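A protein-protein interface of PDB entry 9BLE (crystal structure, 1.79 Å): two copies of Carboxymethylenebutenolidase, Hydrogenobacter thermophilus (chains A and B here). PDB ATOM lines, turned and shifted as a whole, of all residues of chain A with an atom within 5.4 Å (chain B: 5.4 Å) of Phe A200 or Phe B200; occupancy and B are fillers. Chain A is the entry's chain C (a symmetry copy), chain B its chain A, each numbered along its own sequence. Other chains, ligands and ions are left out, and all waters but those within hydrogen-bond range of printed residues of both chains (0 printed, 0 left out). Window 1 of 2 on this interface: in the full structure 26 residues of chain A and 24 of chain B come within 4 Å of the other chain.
O of Leu B201 is in hydrogen-bond range of N of His B172 (2.8 Å).
The side-chain sulfur (SG) of Cys B191 lies within hydrogen-bond range of the backbone carbonyl oxygen (O) of Ala B187, at 3.4 Å.
N of Leu A201 is in hydrogen-bond range of O of Ala A170 (2.9 Å).
N of His A172 sits at hydrogen-bond distance from O of Leu A201, at 2.8 Å.
The backbone NH (N) of Tyr A203 is in hydrogen-bond range of the backbone carbonyl oxygen (O) of His A172, 3.0 Å away.
O of Ala A187 lies within hydrogen-bond range of SG of Cys A191, 3.4 Å away.
Ile A188 touches Ile B202, and with the chains exchanged Ile A202 touches Ile B188.
Ala A198 touches Ser B204, and with the chains exchanged Ser A204 touches Ala B198.
Gln A199 touches Tyr B203, and with the chains exchanged Tyr A203 touches Gln B199.
Phe B200 touches its own counterpart, Phe A200.
Positions printed for both chains: 134, 154, 170, 172, 184, 187, 188, 191, 198, 199, 200, 201, 202, 203 and 204.
Of the 15 printed residues of chain B, 9 touch a printed residue of chain A.
Printed residues of chain B that touch a printed residue of chain A: Ile B188, Cys B191, Ala B198, Gln B199, Phe B200, Leu B201, Ile B202, Tyr B203 and Ser B204.
Of the 15 printed residues of chain A, 9 touch a printed residue of chain B.
Among the printed residues, no Asp or Glu carboxylate lies within 4 Å of a Lys or Arg side-chain nitrogen of the other chain.
Among the printed residues, pairs that only touch across the chains: Ile A188 with Ile B202 (3.8 Å), Cys A191 with Ser B204 (3.5 Å), Ala A198 with Ile B202 (3.8 Å), Ala A198 with Tyr B203 (3.9 Å), Gln A199 with Ile B202 (3.4 Å), Gln A199 with Tyr B203 (3.9 Å), Phe A200 with Leu B201 (3.3 Å), Phe A200 with Ser B204 (3.6 Å), Leu A201 with Phe B200 (3.3 Å), Ile A202 with Ile B188 (3.7 Å), Ile A202 with Ala B198 (3.9 Å), Ile A202 with Gln B199 (3.4 Å), Ile A202 with Ile B202 (3.97 Å), Tyr A203 with Ala B198 (3.96 Å), Tyr A203 with Gln B199 (3.9 Å), Ser A204 with Cys B191 (3.6 Å) and Ser A204 with Phe B200 (3.8 Å).
Of chain B, only Phe B200, Leu B201, Ile B202 and Ser B204 come within 4 Å of Phe A200.
Printed residues of chain A within 4 Å of Tyr B203: Ala A198 (3.9 Å) and Gln A199 (3.9 Å).
Of the printed residues of chain B, Ile A202 touches Ile B188, Ala B198, Gln B199, Phe B200 and Ile B202.
Of the printed residues of chain A, Ala B198 touches Ile A202, Tyr A203 and Ser A204.
Val B184 touches none of the printed residues of chain A.
The nearest residue of chain B that does not touch Phe A200 is Tyr B203 (5.0 Å).
The nearest residue of chain A that does not touch Phe B200 is Tyr A203 (5.0 Å).
O of Ala B198 lies within hydrogen-bond range of OG of Ser A204, at 2.8 Å.
O of Phe B200 lies within hydrogen-bond range of N of Ile A202, at 2.8 Å.
The backbone NH of Ile B202 is in hydrogen-bond range of the backbone carbonyl oxygen of Phe A200, at 2.7 Å.
N of Ser B204 lies within hydrogen-bond range of O of Ala A198 (2.9 Å).
The backbone carbonyl oxygen of Phe B200 lies close to the backbone carbonyl oxygen of Phe A200 (3.4 Å).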
ATOM      1  N   TRP A 134     -24.499  20.067  34.449  1.00  0.00           N
ATOM      2  CA  TRP A 134     -24.912  19.270  33.302  1.00  0.00           C
ATOM      3  C   TRP A 134     -26.210  18.532  33.618  1.00  0.00           C
ATOM      4  O   TRP A 134     -27.150  18.539  32.834  1.00  0.00           O
ATOM      5  CB  TRP A 134     -23.844  18.233  32.939  1.00  0.00           C
ATOM      6  CG  TRP A 134     -22.684  18.671  32.086  1.00  0.00           C
ATOM      7  CD1 TRP A 134     -21.384  18.777  32.487  1.00  0.00           C
ATOM      8  CD2 TRP A 134     -22.683  18.904  30.669  1.00  0.00           C
ATOM      9  NE1 TRP A 134     -20.582  19.118  31.432  1.00  0.00           N
ATOM     10  CE2 TRP A 134     -21.345  19.183  30.306  1.00  0.00           C
ATOM     11  CE3 TRP A 134     -23.665  18.912  29.673  1.00  0.00           C
ATOM     12  CZ2 TRP A 134     -20.972  19.445  28.993  1.00  0.00           C
ATOM     13  CZ3 TRP A 134     -23.284  19.169  28.371  1.00  0.00           C
ATOM     14  CH2 TRP A 134     -21.958  19.415  28.038  1.00  0.00           C
ATOM     15  N   TYR A 154     -18.500  12.947  34.013  1.00  0.00           N
ATOM     16  CA  TYR A 154     -19.608  12.483  33.191  1.00  0.00           C
ATOM     17  C   TYR A 154     -20.012  11.059  33.567  1.00  0.00           C
ATOM     18  O   TYR A 154     -21.033  10.572  33.078  1.00  0.00           O
ATOM     19  CB  TYR A 154     -19.176  12.524  31.724  1.00  0.00           C
ATOM     20  CG  TYR A 154     -18.864  13.932  31.257  1.00  0.00           C
ATOM     21  CD1 TYR A 154     -19.893  14.808  30.950  1.00  0.00           C
ATOM     22  CD2 TYR A 154     -17.563  14.403  31.161  1.00  0.00           C
ATOM     23  CE1 TYR A 154     -19.638  16.106  30.534  1.00  0.00           C
ATOM     24  CE2 TYR A 154     -17.299  15.712  30.769  1.00  0.00           C
ATOM     25  CZ  TYR A 154     -18.337  16.562  30.442  1.00  0.00           C
ATOM     26  OH  TYR A 154     -18.093  17.840  30.009  1.00  0.00           O
ATOM     27  N   ALA A 170     -18.376  24.344  28.467  1.00  0.00           N
ATOM     28  CA  ALA A 170     -17.834  23.318  29.333  1.00  0.00           C
ATOM     29  C   ALA A 170     -16.331  23.509  29.463  1.00  0.00           C
ATOM     30  O   ALA A 170     -15.609  23.383  28.478  1.00  0.00           O
ATOM     31  CB  ALA A 170     -18.155  21.975  28.789  1.00  0.00           C
ATOM     32  N   HIS A 172     -12.633  22.416  30.885  1.00  0.00           N
ATOM     33  CA  HIS A 172     -11.909  21.227  31.277  1.00  0.00           C
ATOM     34  C   HIS A 172     -10.432  21.568  31.449  1.00  0.00           C
ATOM     35  O   HIS A 172      -9.920  22.509  30.825  1.00  0.00           O
ATOM     36  CB  HIS A 172     -12.173  20.041  30.334  1.00  0.00           C
ATOM     37  CG  HIS A 172     -13.522  19.441  30.594  1.00  0.00           C
ATOM     38  ND1 HIS A 172     -13.744  18.699  31.738  1.00  0.00           N
ATOM     39  CD2 HIS A 172     -14.708  19.536  29.968  1.00  0.00           C
ATOM     40  CE1 HIS A 172     -15.021  18.326  31.777  1.00  0.00           C
ATOM     41  NE2 HIS A 172     -15.643  18.838  30.724  1.00  0.00           N
ATOM     42  N   VAL A 184     -13.986  13.540  28.145  1.00  0.00           N
ATOM     43  CA  VAL A 184     -14.398  14.790  27.532  1.00  0.00           C
ATOM     44  C   VAL A 184     -14.784  14.518  26.084  1.00  0.00           C
ATOM     45  O   VAL A 184     -15.804  15.006  25.610  1.00  0.00           O
ATOM     46  CB  VAL A 184     -13.310  15.872  27.673  1.00  0.00           C
ATOM     47  CG1 VAL A 184     -13.724  17.186  27.005  1.00  0.00           C
ATOM     48  CG2 VAL A 184     -12.948  16.119  29.143  1.00  0.00           C
ATOM     49  N   ALA A 187     -18.229  13.131  25.813  1.00  0.00           N
ATOM     50  CA  ALA A 187     -19.220  14.179  25.997  1.00  0.00           C
ATOM     51  C   ALA A 187     -19.385  15.002  24.720  1.00  0.00           C
ATOM     52  O   ALA A 187     -20.510  15.313  24.323  1.00  0.00           O
ATOM     53  CB  ALA A 187     -18.849  15.047  27.187  1.00  0.00           C
ATOM     54  N   ILE A 188     -18.268  15.326  24.053  1.00  0.00           N
ATOM     55  CA  ILE A 188     -18.339  16.060  22.797  1.00  0.00           C
ATOM     56  C   ILE A 188     -19.158  15.258  21.784  1.00  0.00           C
ATOM     57  O   ILE A 188     -20.000  15.804  21.067  1.00  0.00           O
ATOM     58  CB  ILE A 188     -16.930  16.399  22.266  1.00  0.00           C
ATOM     59  CG1 ILE A 188     -16.191  17.344  23.204  1.00  0.00           C
ATOM     60  CG2 ILE A 188     -16.980  16.951  20.838  1.00  0.00           C
ATOM     61  CD1 ILE A 188     -14.690  17.463  22.946  1.00  0.00           C
ATOM     62  N   CYS A 191     -22.801  15.499  22.445  1.00  0.00           N
ATOM     63  CA  CYS A 191     -23.310  16.801  22.058  1.00  0.00           C
ATOM     64  C   CYS A 191     -23.444  16.873  20.535  1.00  0.00           C
ATOM     65  O   CYS A 191     -24.421  17.417  20.033  1.00  0.00           O
ATOM     66  CB  CYS A 191     -22.424  17.915  22.603  1.00  0.00           C
ATOM     67  SG  CYS A 191     -22.516  18.077  24.409  1.00  0.00           S
ATOM     68  N   ALA A 198     -22.796  23.108  22.451  1.00  0.00           N
ATOM     69  CA  ALA A 198     -21.803  23.042  23.508  1.00  0.00           C
ATOM     70  C   ALA A 198     -20.427  23.394  22.965  1.00  0.00           C
ATOM     71  O   ALA A 198     -19.981  22.843  21.954  1.00  0.00           O
ATOM     72  CB  ALA A 198     -21.796  21.669  24.134  1.00  0.00           C
ATOM     73  N   GLN A 199     -19.748  24.298  23.655  1.00  0.00           N
ATOM     74  CA  GLN A 199     -18.358  24.606  23.362  1.00  0.00           C
ATOM     75  C   GLN A 199     -17.525  24.074  24.516  1.00  0.00           C
ATOM     76  O   GLN A 199     -17.860  24.316  25.679  1.00  0.00           O
ATOM     77  CB  GLN A 199     -18.181  26.096  23.070  1.00  0.00           C
ATOM     78  CG  GLN A 199     -18.492  27.008  24.248  1.00  0.00           C
ATOM     79  CD  GLN A 199     -18.413  28.476  23.914  1.00  0.00           C
ATOM     80  OE1 GLN A 199     -17.479  29.158  24.333  1.00  0.00           O
ATOM     81  NE2 GLN A 199     -19.409  28.994  23.218  1.00  0.00           N
ATOM     82  N   PHE A 200     -16.494  23.285  24.181  1.00  0.00           N
ATOM     83  CA  PHE A 200     -15.607  22.695  25.165  1.00  0.00           C
ATOM     84  C   PHE A 200     -14.276  23.434  25.130  1.00  0.00           C
ATOM     85  O   PHE A 200     -13.693  23.625  24.053  1.00  0.00           O
ATOM     86  CB  PHE A 200     -15.369  21.209  24.900  1.00  0.00           C
ATOM     87  CG  PHE A 200     -16.588  20.335  25.164  1.00  0.00           C
ATOM     88  CD1 PHE A 200     -17.658  20.318  24.273  1.00  0.00           C
ATOM     89  CD2 PHE A 200     -16.681  19.585  26.326  1.00  0.00           C
ATOM     90  CE1 PHE A 200     -18.781  19.576  24.544  1.00  0.00           C
ATOM     91  CE2 PHE A 200     -17.823  18.831  26.597  1.00  0.00           C
ATOM     92  CZ  PHE A 200     -18.856  18.813  25.695  1.00  0.00           C
ATOM     93  N   LEU A 201     -13.850  23.930  26.300  1.00  0.00           N
ATOM     94  CA  LEU A 201     -12.653  24.734  26.437  1.00  0.00           C
ATOM     95  C   LEU A 201     -11.693  23.961  27.335  1.00  0.00           C
ATOM     96  O   LEU A 201     -11.991  23.742  28.513  1.00  0.00           O
ATOM     97  CB  LEU A 201     -13.097  26.062  27.038  1.00  0.00           C
ATOM     98  CG  LEU A 201     -12.028  27.102  27.366  1.00  0.00           C
ATOM     99  CD1 LEU A 201     -11.122  27.400  26.188  1.00  0.00           C
ATOM    100  CD2 LEU A 201     -12.762  28.356  27.792  1.00  0.00           C
ATOM    101  N   ILE A 202     -10.582  23.492  26.759  1.00  0.00           N
ATOM    102  CA  ILE A 202      -9.655  22.623  27.461  1.00  0.00           C
ATOM    103  C   ILE A 202      -8.331  23.361  27.587  1.00  0.00           C
ATOM    104  O   ILE A 202      -7.711  23.740  26.561  1.00  0.00           O
ATOM    105  CB  ILE A 202      -9.467  21.289  26.717  1.00  0.00           C
ATOM    106  CG1 ILE A 202     -10.807  20.612  26.445  1.00  0.00           C
ATOM    107  CG2 ILE A 202      -8.522  20.373  27.505  1.00  0.00           C
ATOM    108  CD1 ILE A 202     -10.761  19.470  25.460  1.00  0.00           C
ATOM    109  N   TYR A 203      -7.945  23.621  28.835  1.00  0.00           N
ATOM    110  CA  TYR A 203      -6.722  24.340  29.131  1.00  0.00           C
ATOM    111  C   TYR A 203      -5.592  23.344  29.382  1.00  0.00           C
ATOM    112  O   TYR A 203      -5.639  22.581  30.328  1.00  0.00           O
ATOM    113  CB  TYR A 203      -6.953  25.230  30.352  1.00  0.00           C
ATOM    114  CG  TYR A 203      -7.829  26.442  30.109  1.00  0.00           C
ATOM    115  CD1 TYR A 203      -7.290  27.622  29.607  1.00  0.00           C
ATOM    116  CD2 TYR A 203      -9.188  26.404  30.371  1.00  0.00           C
ATOM    117  CE1 TYR A 203      -8.078  28.736  29.377  1.00  0.00           C
ATOM    118  CE2 TYR A 203      -9.982  27.519  30.167  1.00  0.00           C
ATOM    119  CZ  TYR A 203      -9.424  28.691  29.686  1.00  0.00           C
ATOM    120  OH  TYR A 203     -10.188  29.796  29.476  1.00  0.00           O
ATOM    121  N   SER A 204      -4.558  23.384  28.538  1.00  0.00           N
ATOM    122  CA  SER A 204      -3.409  22.506  28.672  1.00  0.00           C
ATOM    123  C   SER A 204      -2.665  22.798  29.959  1.00  0.00           C
ATOM    124  O   SER A 204      -2.563  23.958  30.372  1.00  0.00           O
ATOM    125  CB  SER A 204      -2.456  22.700  27.510  1.00  0.00           C
ATOM    126  OG  SER A 204      -3.134  22.410  26.302  1.00  0.00           O
ATOM    127  N   TRP B 134       0.441  26.578  13.332  1.00  0.00           N
ATOM    128  CA  TRP B 134       1.157  25.693  14.244  1.00  0.00           C
ATOM    129  C   TRP B 134       2.608  25.509  13.778  1.00  0.00           C
ATOM    130  O   TRP B 134       3.547  25.611  14.562  1.00  0.00           O
ATOM    131  CB  TRP B 134       0.481  24.323  14.339  1.00  0.00           C
ATOM    132  CG  TRP B 134      -0.722  24.200  15.240  1.00  0.00           C
ATOM    133  CD1 TRP B 134      -2.014  23.978  14.840  1.00  0.00           C
ATOM    134  CD2 TRP B 134      -0.727  24.079  16.675  1.00  0.00           C
ATOM    135  NE1 TRP B 134      -2.821  23.785  15.926  1.00  0.00           N
ATOM    136  CE2 TRP B 134      -2.070  23.848  17.062  1.00  0.00           C
ATOM    137  CE3 TRP B 134       0.252  24.153  17.669  1.00  0.00           C
ATOM    138  CZ2 TRP B 134      -2.444  23.658  18.390  1.00  0.00           C
ATOM    139  CZ3 TRP B 134      -0.120  23.982  18.985  1.00  0.00           C
ATOM    140  CH2 TRP B 134      -1.445  23.709  19.333  1.00  0.00           C
ATOM    141  N   TYR B 154      -3.023  18.085  11.902  1.00  0.00           N
ATOM    142  CA  TYR B 154      -1.791  17.826  12.621  1.00  0.00           C
ATOM    143  C   TYR B 154      -0.939  16.778  11.895  1.00  0.00           C
ATOM    144  O   TYR B 154       0.211  16.585  12.272  1.00  0.00           O
ATOM    145  CB  TYR B 154      -2.144  17.349  14.023  1.00  0.00           C
ATOM    146  CG  TYR B 154      -2.831  18.449  14.827  1.00  0.00           C
ATOM    147  CD1 TYR B 154      -2.096  19.471  15.412  1.00  0.00           C
ATOM    148  CD2 TYR B 154      -4.204  18.448  15.014  1.00  0.00           C
ATOM    149  CE1 TYR B 154      -2.700  20.482  16.138  1.00  0.00           C
ATOM    150  CE2 TYR B 154      -4.826  19.465  15.721  1.00  0.00           C
ATOM    151  CZ  TYR B 154      -4.076  20.486  16.275  1.00  0.00           C
ATOM    152  OH  TYR B 154      -4.677  21.502  16.989  1.00  0.00           O
ATOM    153  N   ALA B 170      -6.371  27.321  20.083  1.00  0.00           N
ATOM    154  CA  ALA B 170      -6.598  26.397  18.984  1.00  0.00           C
ATOM    155  C   ALA B 170      -8.083  26.110  18.860  1.00  0.00           C
ATOM    156  O   ALA B 170      -8.664  25.510  19.764  1.00  0.00           O
ATOM    157  CB  ALA B 170      -5.837  25.121  19.212  1.00  0.00           C
ATOM    158  N   HIS B 172     -11.317  24.245  17.109  1.00  0.00           N
ATOM    159  CA  HIS B 172     -11.657  23.023  16.390  1.00  0.00           C
ATOM    160  C   HIS B 172     -13.163  22.901  16.257  1.00  0.00           C
ATOM    161  O   HIS B 172     -13.906  23.430  17.093  1.00  0.00           O
ATOM    162  CB  HIS B 172     -10.981  21.795  17.020  1.00  0.00           C
ATOM    163  CG  HIS B 172      -9.541  21.712  16.661  1.00  0.00           C
ATOM    164  ND1 HIS B 172      -9.162  21.374  15.382  1.00  0.00           N
ATOM    165  CD2 HIS B 172      -8.393  22.062  17.308  1.00  0.00           C
ATOM    166  CE1 HIS B 172      -7.830  21.415  15.282  1.00  0.00           C
ATOM    167  NE2 HIS B 172      -7.334  21.851  16.432  1.00  0.00           N
ATOM    168  N   VAL B 184      -7.188  15.871  17.733  1.00  0.00           N
ATOM    169  CA  VAL B 184      -7.189  17.028  18.619  1.00  0.00           C
ATOM    170  C   VAL B 184      -6.715  16.590  20.007  1.00  0.00           C
ATOM    171  O   VAL B 184      -5.881  17.260  20.624  1.00  0.00           O
ATOM    172  CB  VAL B 184      -8.563  17.727  18.664  1.00  0.00           C
ATOM    173  CG1 VAL B 184      -8.536  18.932  19.596  1.00  0.00           C
ATOM    174  CG2 VAL B 184      -9.044  18.148  17.281  1.00  0.00           C
ATOM    175  N   ALA B 187      -3.014  16.314  20.115  1.00  0.00           N
ATOM    176  CA  ALA B 187      -2.390  17.620  20.189  1.00  0.00           C
ATOM    177  C   ALA B 187      -2.453  18.159  21.617  1.00  0.00           C
ATOM    178  O   ALA B 187      -1.475  18.709  22.108  1.00  0.00           O
ATOM    179  CB  ALA B 187      -3.033  18.572  19.176  1.00  0.00           C
ATOM    180  N   ILE B 188      -3.586  17.969  22.307  1.00  0.00           N
ATOM    181  CA  ILE B 188      -3.692  18.414  23.693  1.00  0.00           C
ATOM    182  C   ILE B 188      -2.630  17.708  24.534  1.00  0.00           C
ATOM    183  O   ILE B 188      -1.960  18.328  25.375  1.00  0.00           O
ATOM    184  CB  ILE B 188      -5.115  18.187  24.247  1.00  0.00           C
ATOM    185  CG1 ILE B 188      -6.127  19.051  23.490  1.00  0.00           C
ATOM    186  CG2 ILE B 188      -5.170  18.417  25.764  1.00  0.00           C
ATOM    187  CD1 ILE B 188      -7.581  18.665  23.731  1.00  0.00           C
ATOM    188  N   CYS B 191       0.748  19.172  23.996  1.00  0.00           N
ATOM    189  CA  CYS B 191       0.846  20.446  24.690  1.00  0.00           C
ATOM    190  C   CYS B 191       1.037  20.228  26.193  1.00  0.00           C
ATOM    191  O   CYS B 191       1.844  20.930  26.815  1.00  0.00           O
ATOM    192  CB  CYS B 191      -0.345  21.335  24.365  1.00  0.00           C
ATOM    193  SG  CYS B 191      -0.367  21.887  22.642  1.00  0.00           S
ATOM    194  N   ALA B 198      -1.475  26.234  25.694  1.00  0.00           N
ATOM    195  CA  ALA B 198      -2.483  26.098  24.665  1.00  0.00           C
ATOM    196  C   ALA B 198      -3.858  25.903  25.295  1.00  0.00           C
ATOM    197  O   ALA B 198      -4.060  25.021  26.137  1.00  0.00           O
ATOM    198  CB  ALA B 198      -2.147  24.970  23.733  1.00  0.00           C
ATOM    199  N   GLN B 199      -4.811  26.726  24.849  1.00  0.00           N
ATOM    200  CA  GLN B 199      -6.210  26.494  25.131  1.00  0.00           C
ATOM    201  C   GLN B 199      -6.901  25.990  23.862  1.00  0.00           C
ATOM    202  O   GLN B 199      -6.702  26.555  22.784  1.00  0.00           O
ATOM    203  CB  GLN B 199      -6.806  27.746  25.745  1.00  0.00           C
ATOM    204  CG  GLN B 199      -6.830  28.952  24.825  1.00  0.00           C
ATOM    205  CD  GLN B 199      -7.312  30.209  25.514  1.00  0.00           C
ATOM    206  OE1 GLN B 199      -8.439  30.646  25.282  1.00  0.00           O
ATOM    207  NE2 GLN B 199      -6.453  30.815  26.326  1.00  0.00           N
ATOM    208  N   PHE B 200      -7.637  24.897  23.998  1.00  0.00           N
ATOM    209  CA  PHE B 200      -8.339  24.263  22.898  1.00  0.00           C
ATOM    210  C   PHE B 200      -9.824  24.524  23.043  1.00  0.00           C
ATOM    211  O   PHE B 200     -10.399  24.258  24.095  1.00  0.00           O
ATOM    212  CB  PHE B 200      -8.077  22.758  22.834  1.00  0.00           C
ATOM    213  CG  PHE B 200      -6.694  22.411  22.316  1.00  0.00           C
ATOM    214  CD1 PHE B 200      -5.603  22.517  23.170  1.00  0.00           C
ATOM    215  CD2 PHE B 200      -6.496  21.942  21.008  1.00  0.00           C
ATOM    216  CE1 PHE B 200      -4.331  22.181  22.711  1.00  0.00           C
ATOM    217  CE2 PHE B 200      -5.210  21.619  20.559  1.00  0.00           C
ATOM    218  CZ  PHE B 200      -4.140  21.745  21.417  1.00  0.00           C
ATOM    219  N   LEU B 201     -10.425  25.055  21.981  1.00  0.00           N
ATOM    220  CA  LEU B 201     -11.834  25.370  21.947  1.00  0.00           C
ATOM    221  C   LEU B 201     -12.516  24.516  20.895  1.00  0.00           C
ATOM    222  O   LEU B 201     -12.194  24.642  19.718  1.00  0.00           O
ATOM    223  CB  LEU B 201     -11.853  26.851  21.623  1.00  0.00           C
ATOM    224  CG  LEU B 201     -13.192  27.557  21.684  1.00  0.00           C
ATOM    225  CD1 LEU B 201     -14.038  27.274  22.901  1.00  0.00           C
ATOM    226  CD2 LEU B 201     -12.860  29.045  21.560  1.00  0.00           C
ATOM    227  N   ILE B 202     -13.402  23.618  21.320  1.00  0.00           N
ATOM    228  CA  ILE B 202     -14.026  22.659  20.410  1.00  0.00           C
ATOM    229  C   ILE B 202     -15.519  22.933  20.385  1.00  0.00           C
ATOM    230  O   ILE B 202     -16.186  22.836  21.417  1.00  0.00           O
ATOM    231  CB  ILE B 202     -13.733  21.198  20.795  1.00  0.00           C
ATOM    232  CG1 ILE B 202     -12.241  20.935  20.955  1.00  0.00           C
ATOM    233  CG2 ILE B 202     -14.370  20.248  19.780  1.00  0.00           C
ATOM    234  CD1 ILE B 202     -11.914  19.642  21.660  1.00  0.00           C
ATOM    235  N   TYR B 203     -16.030  23.325  19.218  1.00  0.00           N
ATOM    236  CA  TYR B 203     -17.422  23.692  19.053  1.00  0.00           C
ATOM    237  C   TYR B 203     -18.209  22.487  18.537  1.00  0.00           C
ATOM    238  O   TYR B 203     -17.974  22.025  17.425  1.00  0.00           O
ATOM    239  CB  TYR B 203     -17.494  24.868  18.074  1.00  0.00           C
ATOM    240  CG  TYR B 203     -17.029  26.196  18.638  1.00  0.00           C
ATOM    241  CD1 TYR B 203     -17.912  27.009  19.328  1.00  0.00           C
ATOM    242  CD2 TYR B 203     -15.724  26.635  18.475  1.00  0.00           C
ATOM    243  CE1 TYR B 203     -17.529  28.233  19.849  1.00  0.00           C
ATOM    244  CE2 TYR B 203     -15.319  27.869  18.973  1.00  0.00           C
ATOM    245  CZ  TYR B 203     -16.219  28.655  19.689  1.00  0.00           C
ATOM    246  OH  TYR B 203     -15.831  29.873  20.166  1.00  0.00           O
ATOM    247  N   SER B 204     -19.153  21.983  19.342  1.00  0.00           N
ATOM    248  CA  SER B 204     -19.932  20.813  18.975  1.00  0.00           C
ATOM    249  C   SER B 204     -20.826  21.125  17.788  1.00  0.00           C
ATOM    250  O   SER B 204     -21.340  22.212  17.671  1.00  0.00           O
ATOM    251  CB  SER B 204     -20.770  20.349  20.150  1.00  0.00           C
ATOM    252  OG  SER B 204     -19.885  19.924  21.172  1.00  0.00           O
